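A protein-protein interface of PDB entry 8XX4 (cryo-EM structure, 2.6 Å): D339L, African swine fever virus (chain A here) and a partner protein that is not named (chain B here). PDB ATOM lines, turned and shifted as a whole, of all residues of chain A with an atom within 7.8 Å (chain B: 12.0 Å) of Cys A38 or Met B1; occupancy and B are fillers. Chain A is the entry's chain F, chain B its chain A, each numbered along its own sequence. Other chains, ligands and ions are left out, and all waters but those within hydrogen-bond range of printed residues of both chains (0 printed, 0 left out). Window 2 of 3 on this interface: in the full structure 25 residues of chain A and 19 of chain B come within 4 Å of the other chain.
The side-chain hydroxyl of Tyr A34 sits at hydrogen-bond distance from the side-chain hydroxyl of Thr A8 (2.4 Å).
Among the printed residues, merely in contact across the chains: Ile A33 with Met B1 (3.2 Å), Thr A9 with Gly B4 (3.2 Å), Ile A33 with Glu B2 (3.2 Å), Thr A9 with Tyr B5 (3.6 Å), Phe A39 with Met B1 (3.7 Å), Tyr A34 with Met B1 (3.9 Å) and Cys A38 with Met B1 (3.9 Å).
Cys A38 touches one residue of chain B. Met B1 touches just these residues of chain A: Ile A33 (3.2 Å), Tyr A34 (3.9 Å), Cys A38 (3.9 Å) and Phe A39 (3.7 Å). Ile A33 touches just these residues of chain B: Met B1 and Glu B2. No residue of chain B comes within 4 Å of Gly A36. Lys A37 touches none of the printed residues of chain B. Phe A39 touches just one residue of chain B: Met B1. No residue of chain B comes within 4 Å of Ser A42. No residue of chain B comes within 4 Å of Phe A43. Of the printed residues of chain A, Glu B2 touches Ile A33 (3.2 Å). Printed residues of chain B within 4 Å of Thr A9: Gly B4 and Tyr B5. Asn A41 touches none of the printed residues of chain B. Ser A78 touches none of the printed residues of chain B. The nearest residue of chain B that does not touch Cys A38 is Glu B2 (10.1 Å). The nearest residue of chain A that does not touch Met B1 is Lys A37 (4.4 Å). The nearest printed residue of chain A that does not touch Tyr B5 is Leu A10 (4.3 Å).
Of the 18 printed residues of chain A, 5 touch a printed residue of chain B. Printed residues of chain A that touch a printed residue of chain B: Thr A9, Ile A33, Tyr A34, Cys A38 and Phe A39. Hydrophobic or aromatic side chains of chain A within 4 Å of the printed part of chain B: Ile A33, Tyr A34 and Phe A39. Among the printed residues, 7 pairs touch across the chains.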
ATOM      1  N   PHE A   6       4.727  20.848  18.593  1.00  0.00           N
ATOM      2  CA  PHE A   6       5.522  19.784  18.005  1.00  0.00           C
ATOM      3  C   PHE A   6       6.717  19.473  18.893  1.00  0.00           C
ATOM      4  O   PHE A   6       7.194  20.325  19.644  1.00  0.00           O
ATOM      5  CB  PHE A   6       6.011  20.160  16.613  1.00  0.00           C
ATOM      6  CG  PHE A   6       4.927  20.219  15.588  1.00  0.00           C
ATOM      7  CD1 PHE A   6       4.484  19.070  14.966  1.00  0.00           C
ATOM      8  CD2 PHE A   6       4.352  21.426  15.244  1.00  0.00           C
ATOM      9  CE1 PHE A   6       3.487  19.124  14.022  1.00  0.00           C
ATOM     10  CE2 PHE A   6       3.357  21.483  14.301  1.00  0.00           C
ATOM     11  CZ  PHE A   6       2.924  20.331  13.688  1.00  0.00           C
ATOM     12  N   THR A   8      10.611  17.719  18.652  1.00  0.00           N
ATOM     13  CA  THR A   8      11.651  17.246  17.757  1.00  0.00           C
ATOM     14  C   THR A   8      12.999  17.361  18.445  1.00  0.00           C
ATOM     15  O   THR A   8      13.175  18.126  19.394  1.00  0.00           O
ATOM     16  CB  THR A   8      11.650  18.025  16.435  1.00  0.00           C
ATOM     17  OG1 THR A   8      12.218  17.213  15.402  1.00  0.00           O
ATOM     18  CG2 THR A   8      12.451  19.304  16.558  1.00  0.00           C
ATOM     19  N   THR A   9      13.946  16.566  17.967  1.00  0.00           N
ATOM     20  CA  THR A   9      15.343  16.689  18.351  1.00  0.00           C
ATOM     21  C   THR A   9      16.118  17.157  17.129  1.00  0.00           C
ATOM     22  O   THR A   9      16.064  16.520  16.074  1.00  0.00           O
ATOM     23  CB  THR A   9      15.896  15.369  18.897  1.00  0.00           C
ATOM     24  OG1 THR A   9      17.325  15.426  18.961  1.00  0.00           O
ATOM     25  CG2 THR A   9      15.470  14.192  18.046  1.00  0.00           C
ATOM     26  N   LEU A  10      16.803  18.285  17.261  1.00  0.00           N
ATOM     27  CA  LEU A  10      17.577  18.832  16.166  1.00  0.00           C
ATOM     28  C   LEU A  10      18.944  18.162  16.114  1.00  0.00           C
ATOM     29  O   LEU A  10      19.299  17.351  16.966  1.00  0.00           O
ATOM     30  CB  LEU A  10      17.720  20.343  16.313  1.00  0.00           C
ATOM     31  CG  LEU A  10      16.491  21.191  16.003  1.00  0.00           C
ATOM     32  CD1 LEU A  10      16.917  22.588  15.634  1.00  0.00           C
ATOM     33  CD2 LEU A  10      15.666  20.575  14.898  1.00  0.00           C
ATOM     34  N   ASN A  32      14.007  26.339   8.974  1.00  0.00           N
ATOM     35  CA  ASN A  32      14.603  25.683   7.818  1.00  0.00           C
ATOM     36  C   ASN A  32      14.065  24.266   7.651  1.00  0.00           C
ATOM     37  O   ASN A  32      13.677  23.880   6.543  1.00  0.00           O
ATOM     38  CB  ASN A  32      16.130  25.706   7.968  1.00  0.00           C
ATOM     39  CG  ASN A  32      16.872  24.946   6.869  1.00  0.00           C
ATOM     40  OD1 ASN A  32      16.404  23.946   6.327  1.00  0.00           O
ATOM     41  ND2 ASN A  32      18.057  25.442   6.535  1.00  0.00           N
ATOM     42  N   ILE A  33      14.017  23.488   8.728  1.00  0.00           N
ATOM     43  CA  ILE A  33      13.586  22.094   8.634  1.00  0.00           C
ATOM     44  C   ILE A  33      12.087  21.967   8.393  1.00  0.00           C
ATOM     45  O   ILE A  33      11.656  21.124   7.606  1.00  0.00           O
ATOM     46  CB  ILE A  33      14.016  21.310   9.888  1.00  0.00           C
ATOM     47  CG1 ILE A  33      15.497  21.531  10.173  1.00  0.00           C
ATOM     48  CG2 ILE A  33      13.718  19.836   9.721  1.00  0.00           C
ATOM     49  CD1 ILE A  33      15.993  20.771  11.364  1.00  0.00           C
ATOM     50  N   TYR A  34      11.259  22.774   9.051  1.00  0.00           N
ATOM     51  CA  TYR A  34       9.812  22.580   9.033  1.00  0.00           C
ATOM     52  C   TYR A  34       9.077  23.721   8.335  1.00  0.00           C
ATOM     53  O   TYR A  34       8.052  24.203   8.817  1.00  0.00           O
ATOM     54  CB  TYR A  34       9.278  22.396  10.450  1.00  0.00           C
ATOM     55  CG  TYR A  34       9.883  21.228  11.188  1.00  0.00           C
ATOM     56  CD1 TYR A  34       9.383  19.946  11.021  1.00  0.00           C
ATOM     57  CD2 TYR A  34      10.948  21.406  12.057  1.00  0.00           C
ATOM     58  CE1 TYR A  34       9.930  18.877  11.693  1.00  0.00           C
ATOM     59  CE2 TYR A  34      11.502  20.343  12.731  1.00  0.00           C
ATOM     60  CZ  TYR A  34      10.989  19.081  12.545  1.00  0.00           C
ATOM     61  OH  TYR A  34      11.538  18.015  13.214  1.00  0.00           O
ATOM     62  N   VAL A  35       9.587  24.163   7.191  1.00  0.00           N
ATOM     63  CA  VAL A  35       8.964  25.221   6.404  1.00  0.00           C
ATOM     64  C   VAL A  35       8.049  24.589   5.362  1.00  0.00           C
ATOM     65  O   VAL A  35       8.517  23.985   4.390  1.00  0.00           O
ATOM     66  CB  VAL A  35      10.016  26.133   5.751  1.00  0.00           C
ATOM     67  CG1 VAL A  35      11.086  25.318   5.023  1.00  0.00           C
ATOM     68  CG2 VAL A  35       9.354  27.120   4.797  1.00  0.00           C
ATOM     69  N   GLY A  36       6.744  24.716   5.573  1.00  0.00           N
ATOM     70  CA  GLY A  36       5.785  24.316   4.560  1.00  0.00           C
ATOM     71  C   GLY A  36       5.884  22.874   4.123  1.00  0.00           C
ATOM     72  O   GLY A  36       5.769  22.588   2.927  1.00  0.00           O
ATOM     73  N   LYS A  37       6.109  21.954   5.054  1.00  0.00           N
ATOM     74  CA  LYS A  37       6.060  20.534   4.755  1.00  0.00           C
ATOM     75  C   LYS A  37       5.229  19.830   5.813  1.00  0.00           C
ATOM     76  O   LYS A  37       5.131  20.285   6.954  1.00  0.00           O
ATOM     77  CB  LYS A  37       7.454  19.906   4.681  1.00  0.00           C
ATOM     78  CG  LYS A  37       8.460  20.482   5.644  1.00  0.00           C
ATOM     79  CD  LYS A  37       9.854  19.967   5.336  1.00  0.00           C
ATOM     80  CE  LYS A  37      10.208  20.128   3.869  1.00  0.00           C
ATOM     81  NZ  LYS A  37      10.141  21.544   3.430  1.00  0.00           N
ATOM     82  N   CYS A  38       4.615  18.721   5.414  1.00  0.00           N
ATOM     83  CA  CYS A  38       3.776  17.969   6.334  1.00  0.00           C
ATOM     84  C   CYS A  38       4.618  17.310   7.418  1.00  0.00           C
ATOM     85  O   CYS A  38       5.670  16.725   7.144  1.00  0.00           O
ATOM     86  CB  CYS A  38       2.971  16.917   5.576  1.00  0.00           C
ATOM     87  SG  CYS A  38       2.348  17.477   3.980  1.00  0.00           S
ATOM     88  N   PHE A  39       4.150  17.412   8.659  1.00  0.00           N
ATOM     89  CA  PHE A  39       4.814  16.757   9.783  1.00  0.00           C
ATOM     90  C   PHE A  39       3.757  16.422  10.823  1.00  0.00           C
ATOM     91  O   PHE A  39       3.200  17.324  11.453  1.00  0.00           O
ATOM     92  CB  PHE A  39       5.906  17.642  10.374  1.00  0.00           C
ATOM     93  CG  PHE A  39       6.650  17.005  11.510  1.00  0.00           C
ATOM     94  CD1 PHE A  39       7.296  15.794  11.336  1.00  0.00           C
ATOM     95  CD2 PHE A  39       6.694  17.609  12.752  1.00  0.00           C
ATOM     96  CE1 PHE A  39       7.977  15.201  12.374  1.00  0.00           C
ATOM     97  CE2 PHE A  39       7.378  17.023  13.798  1.00  0.00           C
ATOM     98  CZ  PHE A  39       8.016  15.815  13.608  1.00  0.00           C
ATOM     99  N   LYS A  40       3.485  15.130  10.990  1.00  0.00           N
ATOM    100  CA  LYS A  40       2.549  14.624  11.992  1.00  0.00           C
ATOM    101  C   LYS A  40       1.136  15.163  11.757  1.00  0.00           C
ATOM    102  O   LYS A  40       0.549  15.839  12.603  1.00  0.00           O
ATOM    103  CB  LYS A  40       3.046  14.936  13.407  1.00  0.00           C
ATOM    104  CG  LYS A  40       4.041  13.909  13.922  1.00  0.00           C
ATOM    105  CD  LYS A  40       4.259  14.018  15.415  1.00  0.00           C
ATOM    106  CE  LYS A  40       5.242  15.120  15.747  1.00  0.00           C
ATOM    107  NZ  LYS A  40       6.507  14.582  16.315  1.00  0.00           N
ATOM    108  N   ASN A  41       0.597  14.832  10.580  1.00  0.00           N
ATOM    109  CA  ASN A  41      -0.777  15.174  10.201  1.00  0.00           C
ATOM    110  C   ASN A  41      -1.026  16.677  10.279  1.00  0.00           C
ATOM    111  O   ASN A  41      -2.045  17.130  10.802  1.00  0.00           O
ATOM    112  CB  ASN A  41      -1.791  14.413  11.056  1.00  0.00           C
ATOM    113  CG  ASN A  41      -2.877  13.757  10.229  1.00  0.00           C
ATOM    114  OD1 ASN A  41      -2.749  13.618   9.014  1.00  0.00           O
ATOM    115  ND2 ASN A  41      -3.956  13.352  10.887  1.00  0.00           N
ATOM    116  N   SER A  42      -0.086  17.457   9.754  1.00  0.00           N
ATOM    117  CA  SER A  42      -0.178  18.908   9.796  1.00  0.00           C
ATOM    118  C   SER A  42       0.796  19.475   8.777  1.00  0.00           C
ATOM    119  O   SER A  42       1.838  18.873   8.519  1.00  0.00           O
ATOM    120  CB  SER A  42       0.139  19.441  11.196  1.00  0.00           C
ATOM    121  OG  SER A  42      -0.875  19.079  12.112  1.00  0.00           O
ATOM    122  N   PHE A  43       0.460  20.631   8.207  1.00  0.00           N
ATOM    123  CA  PHE A  43       1.310  21.231   7.189  1.00  0.00           C
ATOM    124  C   PHE A  43       2.294  22.256   7.739  1.00  0.00           C
ATOM    125  O   PHE A  43       3.248  22.601   7.038  1.00  0.00           O
ATOM    126  CB  PHE A  43       0.461  21.894   6.102  1.00  0.00           C
ATOM    127  CG  PHE A  43       1.266  22.402   4.946  1.00  0.00           C
ATOM    128  CD1 PHE A  43       1.880  21.523   4.077  1.00  0.00           C
ATOM    129  CD2 PHE A  43       1.436  23.759   4.750  1.00  0.00           C
ATOM    130  CE1 PHE A  43       2.631  21.985   3.021  1.00  0.00           C
ATOM    131  CE2 PHE A  43       2.187  24.228   3.696  1.00  0.00           C
ATOM    132  CZ  PHE A  43       2.784  23.342   2.829  1.00  0.00           C
ATOM    133  N   ILE A  44       2.093  22.719   8.976  1.00  0.00           N
ATOM    134  CA  ILE A  44       2.901  23.726   9.676  1.00  0.00           C
ATOM    135  C   ILE A  44       3.390  24.850   8.762  1.00  0.00           C
ATOM    136  O   ILE A  44       4.355  24.692   8.005  1.00  0.00           O
ATOM    137  CB  ILE A  44       4.074  23.074  10.445  1.00  0.00           C
ATOM    138  CG1 ILE A  44       4.971  24.144  11.060  1.00  0.00           C
ATOM    139  CG2 ILE A  44       4.910  22.132   9.585  1.00  0.00           C
ATOM    140  CD1 ILE A  44       6.185  23.572  11.725  1.00  0.00           C
ATOM    141  N   SER A  78      -1.703  23.963   8.801  1.00  0.00           N
ATOM    142  CA  SER A  78      -2.813  24.033   7.856  1.00  0.00           C
ATOM    143  C   SER A  78      -3.412  22.639   7.710  1.00  0.00           C
ATOM    144  O   SER A  78      -3.001  21.859   6.849  1.00  0.00           O
ATOM    145  CB  SER A  78      -2.354  24.567   6.511  1.00  0.00           C
ATOM    146  OG  SER A  78      -1.412  25.605   6.678  1.00  0.00           O
ATOM    147  N   MET B   1      14.160  15.973   6.350  1.00  0.00           N
ATOM    148  CA  MET B   1      13.526  16.612   7.493  1.00  0.00           C
ATOM    149  C   MET B   1      14.422  16.442   8.724  1.00  0.00           C
ATOM    150  O   MET B   1      14.000  16.672   9.854  1.00  0.00           O
ATOM    151  CB  MET B   1      12.128  16.025   7.725  1.00  0.00           C
ATOM    152  CG  MET B   1      11.267  16.766   8.745  1.00  0.00           C
ATOM    153  SD  MET B   1       9.497  16.587   8.467  1.00  0.00           S
ATOM    154  CE  MET B   1       9.481  15.877   6.825  1.00  0.00           C
ATOM    155  N   GLU B   2      15.673  16.043   8.490  1.00  0.00           N
ATOM    156  CA  GLU B   2      16.703  15.990   9.527  1.00  0.00           C
ATOM    157  C   GLU B   2      16.263  15.084  10.683  1.00  0.00           C
ATOM    158  O   GLU B   2      15.873  15.537  11.762  1.00  0.00           O
ATOM    159  CB  GLU B   2      17.070  17.398  10.019  1.00  0.00           C
ATOM    160  CG  GLU B   2      18.087  17.423  11.172  1.00  0.00           C
ATOM    161  CD  GLU B   2      18.866  18.724  11.265  1.00  0.00           C
ATOM    162  OE1 GLU B   2      19.579  19.068  10.299  1.00  0.00           O
ATOM    163  OE2 GLU B   2      18.776  19.395  12.312  1.00  0.00           O
ATOM    164  N   ALA B   3      16.242  13.787  10.388  1.00  0.00           N
ATOM    165  CA  ALA B   3      16.067  12.786  11.434  1.00  0.00           C
ATOM    166  C   ALA B   3      17.019  13.058  12.587  1.00  0.00           C
ATOM    167  O   ALA B   3      18.240  12.978  12.431  1.00  0.00           O
ATOM    168  CB  ALA B   3      16.312  11.390  10.864  1.00  0.00           C
ATOM    169  N   GLY B   4      16.458  13.378  13.748  1.00  0.00           N
ATOM    170  CA  GLY B   4      17.269  13.816  14.861  1.00  0.00           C
ATOM    171  C   GLY B   4      18.043  12.684  15.503  1.00  0.00           C
ATOM    172  O   GLY B   4      17.750  11.505  15.325  1.00  0.00           O
ATOM    173  N   TYR B   5      19.058  13.065  16.271  1.00  0.00           N
ATOM    174  CA  TYR B   5      19.881  12.084  16.960  1.00  0.00           C
ATOM    175  C   TYR B   5      19.070  11.373  18.031  1.00  0.00           C
ATOM    176  O   TYR B   5      18.408  12.011  18.852  1.00  0.00           O
ATOM    177  CB  TYR B   5      21.095  12.765  17.582  1.00  0.00           C
ATOM    178  CG  TYR B   5      21.984  11.844  18.380  1.00  0.00           C
ATOM    179  CD1 TYR B   5      23.021  11.155  17.775  1.00  0.00           C
ATOM    180  CD2 TYR B   5      21.788  11.667  19.739  1.00  0.00           C
ATOM    181  CE1 TYR B   5      23.834  10.321  18.502  1.00  0.00           C
ATOM    182  CE2 TYR B   5      22.594  10.833  20.468  1.00  0.00           C
ATOM    183  CZ  TYR B   5      23.615  10.166  19.847  1.00  0.00           C
ATOM    184  OH  TYR B   5      24.420   9.333  20.578  1.00  0.00           O
ATOM    185  N   ALA B   6      19.138  10.046  18.035  1.00  0.00           N
ATOM    186  CA  ALA B   6      18.406   9.249  18.999  1.00  0.00           C
ATOM    187  C   ALA B   6      19.289   8.112  19.484  1.00  0.00           C
ATOM    188  O   ALA B   6      20.248   7.716  18.821  1.00  0.00           O
ATOM    189  CB  ALA B   6      17.105   8.696  18.408  1.00  0.00           C
ATOM    190  N   HIS B  64      18.965   4.066  -1.706  1.00  0.00           N
ATOM    191  CA  HIS B  64      20.308   4.084  -1.147  1.00  0.00           C
ATOM    192  C   HIS B  64      21.184   3.086  -1.889  1.00  0.00           C
ATOM    193  O   HIS B  64      20.725   2.008  -2.272  1.00  0.00           O
ATOM    194  CB  HIS B  64      20.295   3.756   0.347  1.00  0.00           C
ATOM    195  CG  HIS B  64      20.074   4.949   1.224  1.00  0.00           C
ATOM    196  ND1 HIS B  64      20.813   6.105   1.105  1.00  0.00           N
ATOM    197  CD2 HIS B  64      19.199   5.163   2.233  1.00  0.00           C
ATOM    198  CE1 HIS B  64      20.400   6.981   2.004  1.00  0.00           C
ATOM    199  NE2 HIS B  64      19.422   6.433   2.701  1.00  0.00           N
